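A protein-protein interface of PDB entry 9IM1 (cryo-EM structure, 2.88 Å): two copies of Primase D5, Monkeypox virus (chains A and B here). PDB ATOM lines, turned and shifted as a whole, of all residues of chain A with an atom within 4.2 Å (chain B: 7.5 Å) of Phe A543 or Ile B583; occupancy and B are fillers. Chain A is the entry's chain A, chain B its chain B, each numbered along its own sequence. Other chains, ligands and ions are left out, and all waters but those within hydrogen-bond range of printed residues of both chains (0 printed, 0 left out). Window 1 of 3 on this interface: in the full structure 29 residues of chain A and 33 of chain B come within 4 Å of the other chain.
OD1 of Asn A541 sits close to N of Phe A543, at 3.5 Å.
The backbone carbonyl oxygen (O) of Pro A542 lies close to the side-chain amide oxygen (OD1) of Asn A546, 3.4 Å away.
The backbone NH (N) of Asn B541 lies within hydrogen-bond range of the backbone carbonyl oxygen (O) of Arg B585 (2.8 Å).
The side-chain amide nitrogen (ND2) of Asn B593 sits at hydrogen-bond distance from the side-chain sulfur (SG) of Cys B581, at 3.7 Å.
N of Gly B584 is in hydrogen-bond range of O of Ile B592, 3.1 Å away.
Glu A526 touches Cys B581 (OE1 to CB, 3.8 Å).
O of Glu A526 touches CD1 of Ile B583 (3.5 Å).
CG of Pro A542 touches CD of Arg B585, at 3.5 Å.
Asn B590 touches Pro A542.
Ile B583 touches Phe A543.
Ile B592 touches Phe A543.
ND2 of Asn A546 touches O of Asn B590 (3.9 Å).
Ile B592 touches Asn A546.
Phe A543 touches just these residues of chain B: Ile B583 (3.6 Å) and Ile B592 (3.9 Å).
Of chain A, only Glu A526 and Phe A543 come within 4 Å of Ile B583.
Printed residues of chain A within 4 Å of Ile B592: Phe A543 (3.9 Å) and Asn A546 (3.3 Å).
Of the printed residues of chain B, Pro A542 touches Arg B585 (3.5 Å) and Asn B590 (3.8 Å).
Printed residues of chain A within 4 Å of Asn B590: Pro A542 and Asn A546.
Of the printed residues of chain A, Cys B581 touches Glu A526.
The nearest residue of chain B that does not touch Phe A543 is Asp B537 (4.03 Å).
The nearest residue of chain A that does not touch Ile B583 is Gly A528 (4.02 Å).
Hydrophobic or aromatic side chains of chain B within 4 Å of the printed part of chain A: Ile B583 and Ile B592.
Of the 10 printed residues of chain A, 4 touch a printed residue of chain B.
Printed residues of chain A that touch a printed residue of chain B: Glu A526, Pro A542, Phe A543 and Asn A546.
Among the printed residues, no Asp or Glu carboxylate lies within 4 Å of a Lys or Arg side-chain nitrogen of the other chain.
Positions printed for both chains: 541, 544 and 545.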
ATOM      1  N   GLU A 526       6.948  16.941 -29.855  1.00  0.00           N
ATOM      2  CA  GLU A 526       6.186  17.193 -28.641  1.00  0.00           C
ATOM      3  C   GLU A 526       7.145  17.632 -27.545  1.00  0.00           C
ATOM      4  O   GLU A 526       8.146  16.955 -27.286  1.00  0.00           O
ATOM      5  CB  GLU A 526       5.416  15.941 -28.214  1.00  0.00           C
ATOM      6  CG  GLU A 526       4.535  16.139 -26.998  1.00  0.00           C
ATOM      7  CD  GLU A 526       3.757  14.889 -26.642  1.00  0.00           C
ATOM      8  OE1 GLU A 526       3.930  13.865 -27.335  1.00  0.00           O
ATOM      9  OE2 GLU A 526       2.976  14.930 -25.669  1.00  0.00           O
ATOM     10  N   THR A 527       6.843  18.761 -26.908  1.00  0.00           N
ATOM     11  CA  THR A 527       7.738  19.374 -25.939  1.00  0.00           C
ATOM     12  C   THR A 527       6.948  19.763 -24.696  1.00  0.00           C
ATOM     13  O   THR A 527       5.756  20.073 -24.771  1.00  0.00           O
ATOM     14  CB  THR A 527       8.438  20.606 -26.543  1.00  0.00           C
ATOM     15  OG1 THR A 527       9.126  20.220 -27.737  1.00  0.00           O
ATOM     16  CG2 THR A 527       9.456  21.194 -25.576  1.00  0.00           C
ATOM     17  N   GLY A 528       7.626  19.741 -23.551  1.00  0.00           N
ATOM     18  CA  GLY A 528       6.994  20.076 -22.294  1.00  0.00           C
ATOM     19  C   GLY A 528       6.617  21.541 -22.195  1.00  0.00           C
ATOM     20  O   GLY A 528       6.884  22.358 -23.077  1.00  0.00           O
ATOM     21  N   ASN A 541      19.380  23.976 -22.869  1.00  0.00           N
ATOM     22  CA  ASN A 541      17.942  23.729 -22.943  1.00  0.00           C
ATOM     23  C   ASN A 541      17.658  22.838 -24.143  1.00  0.00           C
ATOM     24  O   ASN A 541      17.292  23.324 -25.222  1.00  0.00           O
ATOM     25  CB  ASN A 541      17.162  25.041 -23.032  1.00  0.00           C
ATOM     26  CG  ASN A 541      15.733  24.900 -22.558  1.00  0.00           C
ATOM     27  OD1 ASN A 541      15.196  23.795 -22.488  1.00  0.00           O
ATOM     28  ND2 ASN A 541      15.106  26.021 -22.227  1.00  0.00           N
ATOM     29  N   PRO A 542      17.825  21.523 -23.995  1.00  0.00           N
ATOM     30  CA  PRO A 542      17.510  20.618 -25.112  1.00  0.00           C
ATOM     31  C   PRO A 542      16.051  20.654 -25.523  1.00  0.00           C
ATOM     32  O   PRO A 542      15.737  20.341 -26.678  1.00  0.00           O
ATOM     33  CB  PRO A 542      17.913  19.240 -24.570  1.00  0.00           C
ATOM     34  CG  PRO A 542      17.886  19.387 -23.096  1.00  0.00           C
ATOM     35  CD  PRO A 542      18.282  20.796 -22.800  1.00  0.00           C
ATOM     36  N   PHE A 543      15.147  21.028 -24.614  1.00  0.00           N
ATOM     37  CA  PHE A 543      13.739  21.143 -24.975  1.00  0.00           C
ATOM     38  C   PHE A 543      13.540  22.183 -26.068  1.00  0.00           C
ATOM     39  O   PHE A 543      12.793  21.955 -27.026  1.00  0.00           O
ATOM     40  CB  PHE A 543      12.909  21.498 -23.741  1.00  0.00           C
ATOM     41  CG  PHE A 543      12.987  20.479 -22.643  1.00  0.00           C
ATOM     42  CD1 PHE A 543      12.301  19.283 -22.739  1.00  0.00           C
ATOM     43  CD2 PHE A 543      13.746  20.720 -21.512  1.00  0.00           C
ATOM     44  CE1 PHE A 543      12.374  18.344 -21.728  1.00  0.00           C
ATOM     45  CE2 PHE A 543      13.822  19.786 -20.498  1.00  0.00           C
ATOM     46  CZ  PHE A 543      13.134  18.597 -20.606  1.00  0.00           C
ATOM     47  N   ILE A 544      14.199  23.334 -25.938  1.00  0.00           N
ATOM     48  CA  ILE A 544      14.174  24.334 -27.000  1.00  0.00           C
ATOM     49  C   ILE A 544      14.982  23.862 -28.202  1.00  0.00           C
ATOM     50  O   ILE A 544      14.575  24.048 -29.355  1.00  0.00           O
ATOM     51  CB  ILE A 544      14.687  25.683 -26.469  1.00  0.00           C
ATOM     52  CG1 ILE A 544      13.777  26.204 -25.358  1.00  0.00           C
ATOM     53  CG2 ILE A 544      14.786  26.693 -27.591  1.00  0.00           C
ATOM     54  CD1 ILE A 544      12.368  26.481 -25.816  1.00  0.00           C
ATOM     55  N   ALA A 545      16.138  23.239 -27.952  1.00  0.00           N
ATOM     56  CA  ALA A 545      17.051  22.891 -29.036  1.00  0.00           C
ATOM     57  C   ALA A 545      16.455  21.859 -29.985  1.00  0.00           C
ATOM     58  O   ALA A 545      16.827  21.821 -31.162  1.00  0.00           O
ATOM     59  CB  ALA A 545      18.368  22.379 -28.462  1.00  0.00           C
ATOM     60  N   ASN A 546      15.540  21.019 -29.503  1.00  0.00           N
ATOM     61  CA  ASN A 546      14.944  20.006 -30.364  1.00  0.00           C
ATOM     62  C   ASN A 546      13.934  20.581 -31.346  1.00  0.00           C
ATOM     63  O   ASN A 546      13.458  19.845 -32.216  1.00  0.00           O
ATOM     64  CB  ASN A 546      14.280  18.918 -29.517  1.00  0.00           C
ATOM     65  CG  ASN A 546      15.289  18.039 -28.810  1.00  0.00           C
ATOM     66  OD1 ASN A 546      16.478  18.066 -29.122  1.00  0.00           O
ATOM     67  ND2 ASN A 546      14.818  17.251 -27.852  1.00  0.00           N
ATOM     68  N   MET A 547      13.600  21.864 -31.235  1.00  0.00           N
ATOM     69  CA  MET A 547      12.643  22.510 -32.121  1.00  0.00           C
ATOM     70  C   MET A 547      13.287  23.064 -33.384  1.00  0.00           C
ATOM     71  O   MET A 547      12.615  23.757 -34.154  1.00  0.00           O
ATOM     72  CB  MET A 547      11.917  23.633 -31.380  1.00  0.00           C
ATOM     73  CG  MET A 547      10.995  23.155 -30.274  1.00  0.00           C
ATOM     74  SD  MET A 547       9.935  24.458 -29.615  1.00  0.00           S
ATOM     75  CE  MET A 547      10.449  25.866 -30.596  1.00  0.00           C
ATOM     76  N   LEU B 536       7.545  17.339 -13.793  1.00  0.00           N
ATOM     77  CA  LEU B 536       8.360  16.297 -14.402  1.00  0.00           C
ATOM     78  C   LEU B 536       9.340  16.820 -15.443  1.00  0.00           C
ATOM     79  O   LEU B 536      10.192  16.055 -15.905  1.00  0.00           O
ATOM     80  CB  LEU B 536       7.461  15.245 -15.059  1.00  0.00           C
ATOM     81  CG  LEU B 536       6.140  14.926 -14.361  1.00  0.00           C
ATOM     82  CD1 LEU B 536       5.151  14.318 -15.342  1.00  0.00           C
ATOM     83  CD2 LEU B 536       6.377  13.997 -13.194  1.00  0.00           C
ATOM     84  N   ASP B 537       9.253  18.096 -15.820  1.00  0.00           N
ATOM     85  CA  ASP B 537      10.000  18.608 -16.964  1.00  0.00           C
ATOM     86  C   ASP B 537      10.892  19.795 -16.607  1.00  0.00           C
ATOM     87  O   ASP B 537      11.258  20.579 -17.488  1.00  0.00           O
ATOM     88  CB  ASP B 537       9.031  18.947 -18.101  1.00  0.00           C
ATOM     89  CG  ASP B 537       8.445  20.339 -17.990  1.00  0.00           C
ATOM     90  OD1 ASP B 537       7.640  20.579 -17.067  1.00  0.00           O
ATOM     91  OD2 ASP B 537       8.773  21.185 -18.842  1.00  0.00           O
ATOM     92  N   LYS B 538      11.273  19.931 -15.339  1.00  0.00           N
ATOM     93  CA  LYS B 538      12.227  20.948 -14.907  1.00  0.00           C
ATOM     94  C   LYS B 538      13.554  20.262 -14.604  1.00  0.00           C
ATOM     95  O   LYS B 538      13.692  19.593 -13.574  1.00  0.00           O
ATOM     96  CB  LYS B 538      11.715  21.705 -13.685  1.00  0.00           C
ATOM     97  CG  LYS B 538      12.316  23.096 -13.528  1.00  0.00           C
ATOM     98  CD  LYS B 538      11.369  24.068 -12.828  1.00  0.00           C
ATOM     99  CE  LYS B 538      10.568  23.414 -11.708  1.00  0.00           C
ATOM    100  NZ  LYS B 538      11.431  22.711 -10.713  1.00  0.00           N
ATOM    101  N   GLY B 539      14.527  20.432 -15.497  1.00  0.00           N
ATOM    102  CA  GLY B 539      15.842  19.868 -15.309  1.00  0.00           C
ATOM    103  C   GLY B 539      15.855  18.360 -15.451  1.00  0.00           C
ATOM    104  O   GLY B 539      14.862  17.741 -15.847  1.00  0.00           O
ATOM    105  N   PRO B 540      16.990  17.739 -15.134  1.00  0.00           N
ATOM    106  CA  PRO B 540      17.068  16.276 -15.189  1.00  0.00           C
ATOM    107  C   PRO B 540      16.137  15.636 -14.171  1.00  0.00           C
ATOM    108  O   PRO B 540      15.902  16.172 -13.087  1.00  0.00           O
ATOM    109  CB  PRO B 540      18.538  15.982 -14.863  1.00  0.00           C
ATOM    110  CG  PRO B 540      19.257  17.276 -15.065  1.00  0.00           C
ATOM    111  CD  PRO B 540      18.272  18.352 -14.753  1.00  0.00           C
ATOM    112  N   ASN B 541      15.603  14.472 -14.535  1.00  0.00           N
ATOM    113  CA  ASN B 541      14.671  13.740 -13.676  1.00  0.00           C
ATOM    114  C   ASN B 541      14.765  12.257 -13.993  1.00  0.00           C
ATOM    115  O   ASN B 541      13.978  11.718 -14.780  1.00  0.00           O
ATOM    116  CB  ASN B 541      13.240  14.246 -13.857  1.00  0.00           C
ATOM    117  CG  ASN B 541      12.339  13.871 -12.700  1.00  0.00           C
ATOM    118  OD1 ASN B 541      11.629  12.869 -12.752  1.00  0.00           O
ATOM    119  ND2 ASN B 541      12.362  14.679 -11.649  1.00  0.00           N
ATOM    120  N   ILE B 544      11.623   9.767 -13.737  1.00  0.00           N
ATOM    121  CA  ILE B 544      10.660   9.642 -14.819  1.00  0.00           C
ATOM    122  C   ILE B 544      11.298   9.088 -16.087  1.00  0.00           C
ATOM    123  O   ILE B 544      10.580   8.516 -16.922  1.00  0.00           O
ATOM    124  CB  ILE B 544       9.971  10.993 -15.110  1.00  0.00           C
ATOM    125  CG1 ILE B 544       8.743  10.818 -16.006  1.00  0.00           C
ATOM    126  CG2 ILE B 544      10.937  11.959 -15.766  1.00  0.00           C
ATOM    127  CD1 ILE B 544       7.876   9.635 -15.647  1.00  0.00           C
ATOM    128  N   ALA B 545      12.611   9.214 -16.251  1.00  0.00           N
ATOM    129  CA  ALA B 545      13.294   8.714 -17.434  1.00  0.00           C
ATOM    130  C   ALA B 545      13.766   7.275 -17.293  1.00  0.00           C
ATOM    131  O   ALA B 545      14.231   6.696 -18.280  1.00  0.00           O
ATOM    132  CB  ALA B 545      14.490   9.608 -17.767  1.00  0.00           C
ATOM    133  N   LYS B 576      -0.633  13.293 -17.991  1.00  0.00           N
ATOM    134  CA  LYS B 576       0.559  13.069 -18.800  1.00  0.00           C
ATOM    135  C   LYS B 576       1.038  11.628 -18.706  1.00  0.00           C
ATOM    136  O   LYS B 576       1.647  11.116 -19.651  1.00  0.00           O
ATOM    137  CB  LYS B 576       1.671  14.023 -18.373  1.00  0.00           C
ATOM    138  CG  LYS B 576       1.359  15.485 -18.618  1.00  0.00           C
ATOM    139  CD  LYS B 576       2.492  16.373 -18.138  1.00  0.00           C
ATOM    140  CE  LYS B 576       2.160  17.841 -18.332  1.00  0.00           C
ATOM    141  NZ  LYS B 576       1.015  18.261 -17.483  1.00  0.00           N
ATOM    142  N   CYS B 581       3.510   9.078 -24.957  1.00  0.00           N
ATOM    143  CA  CYS B 581       4.844   9.651 -24.844  1.00  0.00           C
ATOM    144  C   CYS B 581       4.920  10.526 -23.603  1.00  0.00           C
ATOM    145  O   CYS B 581       4.006  11.313 -23.336  1.00  0.00           O
ATOM    146  CB  CYS B 581       5.209  10.461 -26.089  1.00  0.00           C
ATOM    147  SG  CYS B 581       5.358   9.475 -27.593  1.00  0.00           S
ATOM    148  N   VAL B 582       6.007  10.384 -22.850  1.00  0.00           N
ATOM    149  CA  VAL B 582       6.233  11.141 -21.627  1.00  0.00           C
ATOM    150  C   VAL B 582       7.523  11.931 -21.793  1.00  0.00           C
ATOM    151  O   VAL B 582       8.535  11.389 -22.256  1.00  0.00           O
ATOM    152  CB  VAL B 582       6.298  10.221 -20.394  1.00  0.00           C
ATOM    153  CG1 VAL B 582       6.603  11.023 -19.141  1.00  0.00           C
ATOM    154  CG2 VAL B 582       4.992   9.459 -20.238  1.00  0.00           C
ATOM    155  N   ILE B 583       7.478  13.214 -21.451  1.00  0.00           N
ATOM    156  CA  ILE B 583       8.627  14.100 -21.596  1.00  0.00           C
ATOM    157  C   ILE B 583       9.462  14.038 -20.324  1.00  0.00           C
ATOM    158  O   ILE B 583       8.978  14.358 -19.234  1.00  0.00           O
ATOM    159  CB  ILE B 583       8.186  15.538 -21.896  1.00  0.00           C
ATOM    160  CG1 ILE B 583       7.282  15.569 -23.126  1.00  0.00           C
ATOM    161  CG2 ILE B 583       9.397  16.430 -22.108  1.00  0.00           C
ATOM    162  CD1 ILE B 583       7.940  15.039 -24.380  1.00  0.00           C
ATOM    163  N   GLY B 584      10.718  13.631 -20.466  1.00  0.00           N
ATOM    164  CA  GLY B 584      11.634  13.573 -19.343  1.00  0.00           C
ATOM    165  C   GLY B 584      13.052  13.425 -19.838  1.00  0.00           C
ATOM    166  O   GLY B 584      13.293  12.964 -20.959  1.00  0.00           O
ATOM    167  N   ARG B 585      13.998  13.813 -18.980  1.00  0.00           N
ATOM    168  CA  ARG B 585      15.396  13.863 -19.383  1.00  0.00           C
ATOM    169  C   ARG B 585      16.318  13.260 -18.329  1.00  0.00           C
ATOM    170  O   ARG B 585      16.252  13.655 -17.151  1.00  0.00           O
ATOM    171  CB  ARG B 585      15.805  15.308 -19.669  1.00  0.00           C
ATOM    172  CG  ARG B 585      17.223  15.451 -20.178  1.00  0.00           C
ATOM    173  CD  ARG B 585      17.470  16.841 -20.719  1.00  0.00           C
ATOM    174  NE  ARG B 585      17.680  17.819 -19.659  1.00  0.00           N
ATOM    175  CZ  ARG B 585      18.856  18.083 -19.110  1.00  0.00           C
ATOM    176  NH1 ARG B 585      19.953  17.449 -19.490  1.00  0.00           N
ATOM    177  NH2 ARG B 585      18.935  19.005 -18.157  1.00  0.00           N
ATOM    178  N   ASN B 590      20.320  14.247 -23.897  1.00  0.00           N
ATOM    179  CA  ASN B 590      19.485  15.130 -24.696  1.00  0.00           C
ATOM    180  C   ASN B 590      18.168  14.496 -25.116  1.00  0.00           C
ATOM    181  O   ASN B 590      17.314  15.196 -25.673  1.00  0.00           O
ATOM    182  CB  ASN B 590      20.240  15.591 -25.953  1.00  0.00           C
ATOM    183  CG  ASN B 590      21.429  16.467 -25.628  1.00  0.00           C
ATOM    184  OD1 ASN B 590      21.287  17.669 -25.408  1.00  0.00           O
ATOM    185  ND2 ASN B 590      22.613  15.870 -25.600  1.00  0.00           N
ATOM    186  N   LYS B 591      17.981  13.202 -24.875  1.00  0.00           N
ATOM    187  CA  LYS B 591      16.743  12.531 -25.244  1.00  0.00           C
ATOM    188  C   LYS B 591      15.635  12.927 -24.277  1.00  0.00           C
ATOM    189  O   LYS B 591      15.784  12.783 -23.059  1.00  0.00           O
ATOM    190  CB  LYS B 591      16.949  11.021 -25.242  1.00  0.00           C
ATOM    191  CG  LYS B 591      17.996  10.549 -26.233  1.00  0.00           C
ATOM    192  CD  LYS B 591      18.719   9.316 -25.725  1.00  0.00           C
ATOM    193  CE  LYS B 591      20.006   9.078 -26.495  1.00  0.00           C
ATOM    194  NZ  LYS B 591      20.303   7.627 -26.643  1.00  0.00           N
ATOM    195  N   ILE B 592      14.523  13.424 -24.816  1.00  0.00           N
ATOM    196  CA  ILE B 592      13.425  13.943 -24.009  1.00  0.00           C
ATOM    197  C   ILE B 592      12.148  13.139 -24.170  1.00  0.00           C
ATOM    198  O   ILE B 592      11.151  13.447 -23.503  1.00  0.00           O
ATOM    199  CB  ILE B 592      13.160  15.427 -24.320  1.00  0.00           C
ATOM    200  CG1 ILE B 592      12.497  15.571 -25.691  1.00  0.00           C
ATOM    201  CG2 ILE B 592      14.453  16.220 -24.266  1.00  0.00           C
ATOM    202  CD1 ILE B 592      12.048  16.977 -26.006  1.00  0.00           C
ATOM    203  N   ASN B 593      12.140  12.121 -25.024  1.00  0.00           N
ATOM    204  CA  ASN B 593      10.947  11.333 -25.301  1.00  0.00           C
ATOM    205  C   ASN B 593      11.079   9.956 -24.666  1.00  0.00           C
ATOM    206  O   ASN B 593      12.107   9.290 -24.831  1.00  0.00           O
ATOM    207  CB  ASN B 593      10.725  11.200 -26.808  1.00  0.00           C
ATOM    208  CG  ASN B 593       9.277  10.943 -27.161  1.00  0.00           C
ATOM    209  OD1 ASN B 593       8.382  11.657 -26.711  1.00  0.00           O
ATOM    210  ND2 ASN B 593       9.039   9.919 -27.971  1.00  0.00           N
ATOM    211  N   ASN B 594      10.042   9.531 -23.945  1.00  0.00           N
ATOM    212  CA  ASN B 594      10.001   8.202 -23.354  1.00  0.00           C
ATOM    213  C   ASN B 594       8.705   7.516 -23.755  1.00  0.00           C
ATOM    214  O   ASN B 594       7.631   8.122 -23.705  1.00  0.00           O
ATOM    215  CB  ASN B 594      10.114   8.273 -21.827  1.00  0.00           C
ATOM    216  CG  ASN B 594      11.245   9.173 -21.366  1.00  0.00           C
ATOM    217  OD1 ASN B 594      12.409   8.775 -21.361  1.00  0.00           O
ATOM    218  ND2 ASN B 594      10.907  10.396 -20.982  1.00  0.00           N
